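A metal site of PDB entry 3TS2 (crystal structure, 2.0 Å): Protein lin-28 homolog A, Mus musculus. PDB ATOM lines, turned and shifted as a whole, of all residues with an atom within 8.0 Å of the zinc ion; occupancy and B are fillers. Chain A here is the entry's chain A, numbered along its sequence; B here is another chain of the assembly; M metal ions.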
ATOM      1  N   VAL A  85      34.932 -18.091   4.128  1.00  0.00           N
ATOM      2  CA  VAL A  85      33.578 -17.924   4.670  1.00  0.00           C
ATOM      3  C   VAL A  85      33.017 -16.501   4.343  1.00  0.00           C
ATOM      4  O   VAL A  85      33.778 -15.629   3.911  1.00  0.00           O
ATOM      5  CB  VAL A  85      33.496 -18.226   6.207  1.00  0.00           C
ATOM      6  CG1 VAL A  85      34.020 -19.634   6.531  1.00  0.00           C
ATOM      7  CG2 VAL A  85      34.202 -17.169   7.048  1.00  0.00           C
ATOM      8  N   PHE A  86      31.691 -16.286   4.517  1.00  0.00           N
ATOM      9  CA  PHE A  86      31.123 -14.935   4.310  1.00  0.00           C
ATOM     10  C   PHE A  86      31.693 -13.935   5.324  1.00  0.00           C
ATOM     11  O   PHE A  86      31.994 -14.310   6.477  1.00  0.00           O
ATOM     12  CB  PHE A  86      29.576 -14.940   4.386  1.00  0.00           C
ATOM     13  CG  PHE A  86      28.872 -15.863   3.405  1.00  0.00           C
ATOM     14  CD1 PHE A  86      29.035 -15.700   2.030  1.00  0.00           C
ATOM     15  CD2 PHE A  86      27.992 -16.836   3.850  1.00  0.00           C
ATOM     16  CE1 PHE A  86      28.410 -16.573   1.123  1.00  0.00           C
ATOM     17  CE2 PHE A  86      27.344 -17.687   2.934  1.00  0.00           C
ATOM     18  CZ  PHE A  86      27.569 -17.553   1.584  1.00  0.00           C
ATOM     19  N   ARG A  99      21.819 -18.295  11.008  1.00  0.00           N
ATOM     20  CA  ARG A  99      23.048 -18.366  10.237  1.00  0.00           C
ATOM     21  C   ARG A  99      23.611 -19.798  10.377  1.00  0.00           C
ATOM     22  O   ARG A  99      23.487 -20.406  11.448  1.00  0.00           O
ATOM     23  CB  ARG A  99      24.073 -17.340  10.753  1.00  0.00           C
ATOM     24  CG  ARG A  99      23.721 -15.908  10.421  1.00  0.00           C
ATOM     25  CD  ARG A  99      24.886 -14.976  10.746  1.00  0.00           C
ATOM     26  NE  ARG A  99      25.269 -14.150   9.594  1.00  0.00           N
ATOM     27  CZ  ARG A  99      26.519 -13.988   9.180  1.00  0.00           C
ATOM     28  NH1 ARG A  99      26.780 -13.227   8.119  1.00  0.00           N
ATOM     29  NH2 ARG A  99      27.533 -14.584   9.810  1.00  0.00           N
ATOM     30  N   CYS A 100      24.235 -20.328   9.296  1.00  0.00           N
ATOM     31  CA  CYS A 100      24.900 -21.638   9.321  1.00  0.00           C
ATOM     32  C   CYS A 100      26.080 -21.515  10.300  1.00  0.00           C
ATOM     33  O   CYS A 100      26.818 -20.547  10.223  1.00  0.00           O
ATOM     34  CB  CYS A 100      25.392 -22.003   7.920  1.00  0.00           C
ATOM     35  SG  CYS A 100      26.656 -23.314   7.909  1.00  0.00           S
ATOM     36  N   TYR A 101      26.238 -22.471  11.227  1.00  0.00           N
ATOM     37  CA  TYR A 101      27.344 -22.347  12.184  1.00  0.00           C
ATOM     38  C   TYR A 101      28.773 -22.505  11.583  1.00  0.00           C
ATOM     39  O   TYR A 101      29.740 -22.052  12.188  1.00  0.00           O
ATOM     40  CB  TYR A 101      27.111 -23.212  13.435  1.00  0.00           C
ATOM     41  CG  TYR A 101      25.867 -22.831  14.222  1.00  0.00           C
ATOM     42  CD1 TYR A 101      25.506 -21.501  14.394  1.00  0.00           C
ATOM     43  CD2 TYR A 101      25.078 -23.812  14.824  1.00  0.00           C
ATOM     44  CE1 TYR A 101      24.367 -21.143  15.111  1.00  0.00           C
ATOM     45  CE2 TYR A 101      23.932 -23.467  15.558  1.00  0.00           C
ATOM     46  CZ  TYR A 101      23.587 -22.134  15.693  1.00  0.00           C
ATOM     47  OH  TYR A 101      22.458 -21.777  16.401  1.00  0.00           O
ATOM     48  N   ASN A 102      28.878 -23.063  10.361  1.00  0.00           N
ATOM     49  CA  ASN A 102      30.173 -23.320   9.699  1.00  0.00           C
ATOM     50  C   ASN A 102      30.709 -22.202   8.771  1.00  0.00           C
ATOM     51  O   ASN A 102      31.893 -21.863   8.843  1.00  0.00           O
ATOM     52  CB  ASN A 102      30.076 -24.645   8.947  1.00  0.00           C
ATOM     53  CG  ASN A 102      31.404 -25.172   8.518  1.00  0.00           C
ATOM     54  OD1 ASN A 102      32.298 -25.437   9.335  1.00  0.00           O
ATOM     55  ND2 ASN A 102      31.550 -25.352   7.219  1.00  0.00           N
ATOM     56  N   CYS A 103      29.834 -21.665   7.895  1.00  0.00           N
ATOM     57  CA  CYS A 103      30.134 -20.670   6.855  1.00  0.00           C
ATOM     58  C   CYS A 103      29.457 -19.309   7.084  1.00  0.00           C
ATOM     59  O   CYS A 103      29.859 -18.319   6.472  1.00  0.00           O
ATOM     60  CB  CYS A 103      29.776 -21.229   5.474  1.00  0.00           C
ATOM     61  SG  CYS A 103      27.995 -21.110   5.072  1.00  0.00           S
ATOM     62  N   GLY A 104      28.364 -19.302   7.856  1.00  0.00           N
ATOM     63  CA  GLY A 104      27.621 -18.087   8.150  1.00  0.00           C
ATOM     64  C   GLY A 104      26.473 -17.750   7.222  1.00  0.00           C
ATOM     65  O   GLY A 104      25.886 -16.670   7.331  1.00  0.00           O
ATOM     66  N   GLY A 105      26.148 -18.660   6.306  1.00  0.00           N
ATOM     67  CA  GLY A 105      25.055 -18.459   5.352  1.00  0.00           C
ATOM     68  C   GLY A 105      23.677 -18.541   5.998  1.00  0.00           C
ATOM     69  O   GLY A 105      23.551 -19.156   7.056  1.00  0.00           O
ATOM     70  N   LEU A 106      22.632 -17.938   5.384  1.00  0.00           N
ATOM     71  CA  LEU A 106      21.251 -17.994   5.932  1.00  0.00           C
ATOM     72  C   LEU A 106      20.432 -19.169   5.338  1.00  0.00           C
ATOM     73  O   LEU A 106      19.455 -19.633   5.926  1.00  0.00           O
ATOM     74  CB  LEU A 106      20.505 -16.662   5.681  1.00  0.00           C
ATOM     75  CG  LEU A 106      21.255 -15.378   6.078  1.00  0.00           C
ATOM     76  CD1 LEU A 106      20.894 -14.231   5.143  1.00  0.00           C
ATOM     77  CD2 LEU A 106      20.970 -14.974   7.530  1.00  0.00           C
ATOM     78  N   ASP A 107      20.853 -19.606   4.159  1.00  0.00           N
ATOM     79  CA  ASP A 107      20.344 -20.665   3.288  1.00  0.00           C
ATOM     80  C   ASP A 107      20.102 -22.043   3.967  1.00  0.00           C
ATOM     81  O   ASP A 107      19.218 -22.785   3.548  1.00  0.00           O
ATOM     82  CB  ASP A 107      21.485 -20.877   2.249  1.00  0.00           C
ATOM     83  CG  ASP A 107      21.106 -21.425   0.898  1.00  0.00           C
ATOM     84  OD1 ASP A 107      20.717 -20.625   0.027  1.00  0.00           O
ATOM     85  OD2 ASP A 107      21.323 -22.641   0.672  1.00  0.00           O
ATOM     86  N   HIS A 108      20.965 -22.404   4.946  1.00  0.00           N
ATOM     87  CA  HIS A 108      21.030 -23.743   5.528  1.00  0.00           C
ATOM     88  C   HIS A 108      21.660 -23.759   6.937  1.00  0.00           C
ATOM     89  O   HIS A 108      22.110 -22.733   7.462  1.00  0.00           O
ATOM     90  CB  HIS A 108      21.961 -24.575   4.605  1.00  0.00           C
ATOM     91  CG  HIS A 108      23.338 -23.958   4.503  1.00  0.00           C
ATOM     92  ND1 HIS A 108      23.563 -22.786   3.793  1.00  0.00           N
ATOM     93  CD2 HIS A 108      24.482 -24.281   5.165  1.00  0.00           C
ATOM     94  CE1 HIS A 108      24.843 -22.480   3.978  1.00  0.00           C
ATOM     95  NE2 HIS A 108      25.435 -23.353   4.785  1.00  0.00           N
ATOM     96  N   HIS A 109      21.769 -24.973   7.477  1.00  0.00           N
ATOM     97  CA  HIS A 109      22.383 -25.293   8.764  1.00  0.00           C
ATOM     98  C   HIS A 109      23.696 -26.057   8.514  1.00  0.00           C
ATOM     99  O   HIS A 109      23.871 -26.600   7.430  1.00  0.00           O
ATOM    100  CB  HIS A 109      21.388 -26.058   9.652  1.00  0.00           C
ATOM    101  CG  HIS A 109      20.257 -25.189  10.168  1.00  0.00           C
ATOM    102  ND1 HIS A 109      19.228 -25.720  10.920  1.00  0.00           N
ATOM    103  CD2 HIS A 109      20.058 -23.846  10.040  1.00  0.00           C
ATOM    104  CE1 HIS A 109      18.435 -24.707  11.220  1.00  0.00           C
ATOM    105  NE2 HIS A 109      18.884 -23.558  10.696  1.00  0.00           N
ATOM    106  N   ALA A 110      24.624 -26.046   9.492  1.00  0.00           N
ATOM    107  CA  ALA A 110      25.967 -26.652   9.401  1.00  0.00           C
ATOM    108  C   ALA A 110      26.052 -28.055   8.809  1.00  0.00           C
ATOM    109  O   ALA A 110      26.996 -28.342   8.063  1.00  0.00           O
ATOM    110  CB  ALA A 110      26.680 -26.585  10.747  1.00  0.00           C
ATOM    111  N   LYS A 111      25.058 -28.919   9.081  1.00  0.00           N
ATOM    112  CA  LYS A 111      24.979 -30.306   8.589  1.00  0.00           C
ATOM    113  C   LYS A 111      24.852 -30.330   7.048  1.00  0.00           C
ATOM    114  O   LYS A 111      25.430 -31.202   6.390  1.00  0.00           O
ATOM    115  CB  LYS A 111      23.780 -31.067   9.207  1.00  0.00           C
ATOM    116  CG  LYS A 111      23.370 -30.630  10.635  1.00  0.00           C
ATOM    117  CD  LYS A 111      22.280 -29.523  10.667  1.00  0.00           C
ATOM    118  CE  LYS A 111      20.864 -30.065  10.704  1.00  0.00           C
ATOM    119  NZ  LYS A 111      19.856 -28.988  10.909  1.00  0.00           N
ATOM    120  N   GLU A 112      24.118 -29.353   6.484  1.00  0.00           N
ATOM    121  CA  GLU A 112      23.876 -29.214   5.039  1.00  0.00           C
ATOM    122  C   GLU A 112      24.948 -28.323   4.362  1.00  0.00           C
ATOM    123  O   GLU A 112      24.882 -28.132   3.140  1.00  0.00           O
ATOM    124  CB  GLU A 112      22.477 -28.579   4.796  1.00  0.00           C
ATOM    125  CG  GLU A 112      21.248 -29.378   5.217  1.00  0.00           C
ATOM    126  CD  GLU A 112      21.030 -29.709   6.686  1.00  0.00           C
ATOM    127  OE1 GLU A 112      20.554 -28.827   7.456  1.00  0.00           O
ATOM    128  OE2 GLU A 112      21.291 -30.874   7.064  1.00  0.00           O
ATOM    129  N   CYS A 113      25.914 -27.759   5.142  1.00  0.00           N
ATOM    130  CA  CYS A 113      26.943 -26.869   4.582  1.00  0.00           C
ATOM    131  C   CYS A 113      27.804 -27.530   3.525  1.00  0.00           C
ATOM    132  O   CYS A 113      28.303 -28.625   3.739  1.00  0.00           O
ATOM    133  CB  CYS A 113      27.787 -26.217   5.678  1.00  0.00           C
ATOM    134  SG  CYS A 113      28.784 -24.796   5.110  1.00  0.00           S
ATOM    135  N   LYS A 114      27.961 -26.858   2.369  1.00  0.00           N
ATOM    136  CA  LYS A 114      28.784 -27.334   1.248  1.00  0.00           C
ATOM    137  C   LYS A 114      30.269 -26.955   1.398  1.00  0.00           C
ATOM    138  O   LYS A 114      31.107 -27.470   0.674  1.00  0.00           O
ATOM    139  CB  LYS A 114      28.217 -26.914  -0.115  1.00  0.00           C
ATOM    140  CG  LYS A 114      26.855 -27.535  -0.455  1.00  0.00           C
ATOM    141  CD  LYS A 114      26.221 -26.815  -1.639  1.00  0.00           C
ATOM    142  CE  LYS A 114      24.760 -27.150  -1.869  1.00  0.00           C
ATOM    143  NZ  LYS A 114      24.064 -26.071  -2.633  1.00  0.00           N
ATOM    144  N   LEU A 115      30.594 -26.065   2.351  1.00  0.00           N
ATOM    145  CA  LEU A 115      31.971 -25.711   2.633  1.00  0.00           C
ATOM    146  C   LEU A 115      32.666 -26.767   3.526  1.00  0.00           C
ATOM    147  O   LEU A 115      31.999 -27.471   4.283  1.00  0.00           O
ATOM    148  CB  LEU A 115      32.035 -24.352   3.303  1.00  0.00           C
ATOM    149  CG  LEU A 115      32.295 -23.194   2.379  1.00  0.00           C
ATOM    150  CD1 LEU A 115      31.022 -22.567   1.888  1.00  0.00           C
ATOM    151  CD2 LEU A 115      33.181 -22.229   3.088  1.00  0.00           C
ATOM    152  N   PRO A 116      34.001 -26.945   3.411  1.00  0.00           N
ATOM    153  CA  PRO A 116      34.667 -27.942   4.289  1.00  0.00           C
ATOM    154  C   PRO A 116      34.489 -27.558   5.787  1.00  0.00           C
ATOM    155  O   PRO A 116      34.195 -26.414   6.069  1.00  0.00           O
ATOM    156  CB  PRO A 116      36.152 -27.846   3.860  1.00  0.00           C
ATOM    157  CG  PRO A 116      36.188 -27.057   2.644  1.00  0.00           C
ATOM    158  CD  PRO A 116      34.973 -26.228   2.572  1.00  0.00           C
ATOM    159  N   GLN A 118      35.005 -25.828   9.137  1.00  0.00           N
ATOM    160  CA  GLN A 118      35.810 -24.646   9.420  1.00  0.00           C
ATOM    161  C   GLN A 118      36.240 -24.616  10.867  1.00  0.00           C
ATOM    162  O   GLN A 118      35.450 -25.044  11.718  1.00  0.00           O
ATOM    163  CB  GLN A 118      35.030 -23.341   9.065  1.00  0.00           C
ATOM    164  CG  GLN A 118      34.761 -23.176   7.558  1.00  0.00           C
ATOM    165  CD  GLN A 118      36.022 -23.072   6.743  1.00  0.00           C
ATOM    166  OE1 GLN A 118      36.904 -22.304   7.063  1.00  0.00           O
ATOM    167  NE2 GLN A 118      36.114 -23.821   5.647  1.00  0.00           N
ATOM    168  P     G B  24      22.109 -29.716  16.664  1.00  0.00           P
ATOM    169  OP1   G B  24      22.227 -31.195  16.712  1.00  0.00           O
ATOM    170  OP2   G B  24      22.679 -28.985  15.514  1.00  0.00           O
ATOM    171  O5'   G B  24      20.551 -29.341  16.779  1.00  0.00           O
ATOM    172  C5'   G B  24      20.101 -28.116  17.371  1.00  0.00           C
ATOM    173  C4'   G B  24      19.060 -27.358  16.571  1.00  0.00           C
ATOM    174  O4'   G B  24      19.627 -26.058  16.271  1.00  0.00           O
ATOM    175  C3'   G B  24      18.605 -27.932  15.224  1.00  0.00           C
ATOM    176  O3'   G B  24      17.481 -28.804  15.339  1.00  0.00           O
ATOM    177  C2'   G B  24      18.320 -26.684  14.383  1.00  0.00           C
ATOM    178  O2'   G B  24      17.032 -26.136  14.575  1.00  0.00           O
ATOM    179  C1'   G B  24      19.392 -25.724  14.915  1.00  0.00           C
ATOM    180  N9    G B  24      20.634 -25.687  14.135  1.00  0.00           N
ATOM    181  C8    G B  24      21.411 -26.740  13.712  1.00  0.00           C
ATOM    182  N7    G B  24      22.421 -26.383  12.976  1.00  0.00           N
ATOM    183  C5    G B  24      22.321 -25.001  12.891  1.00  0.00           C
ATOM    184  C6    G B  24      23.108 -24.046  12.180  1.00  0.00           C
ATOM    185  O6    G B  24      24.140 -24.258  11.525  1.00  0.00           O
ATOM    186  N1    G B  24      22.651 -22.737  12.364  1.00  0.00           N
ATOM    187  C2    G B  24      21.527 -22.390  13.102  1.00  0.00           C
ATOM    188  N2    G B  24      21.217 -21.085  13.206  1.00  0.00           N
ATOM    189  N3    G B  24      20.774 -23.276  13.749  1.00  0.00           N
ATOM    190  C4    G B  24      21.218 -24.555  13.600  1.00  0.00           C
HETATM  191 ZN    ZN M   1      27.288 -23.158   5.712  1.00  0.00          ZN
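The side-chain sulfur (SG) of Cys 103 sits close to the backbone NH (N) of Gly 105, at 3.3 Å. O of Cys 103 is in hydrogen-bond range of N of Phe 86 (3.4 Å). SG of Cys 100 sits close to N of Asn 102, 3.3 Å away. N of Cys 100 lies within hydrogen-bond range of O of Gly 105 (2.6 Å). The backbone NH (N) of Ala 110 sits close to the side-chain sulfur (SG) of Cys 100 (3.8 Å). The side-chain sulfur of Cys 113 lies close to the side-chain amide nitrogen of Asn 102 (3.5 Å). The side-chain sulfur (SG) of Cys 113 sits close to the backbone NH (N) of Leu 115, at 3.5 Å.
Within 4 Å of the zinc ion: Cys 100, Cys 103, His 108 and Cys 113.
NE2 of His 108 is bound to the zinc ion (2.1 Å). SG of Cys 103 is bound to the zinc ion (2.3 Å). The zinc ion is bound by SG of Cys 100, 2.3 Å away. SG of Cys 113 is bound to the zinc ion, at 2.3 Å.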
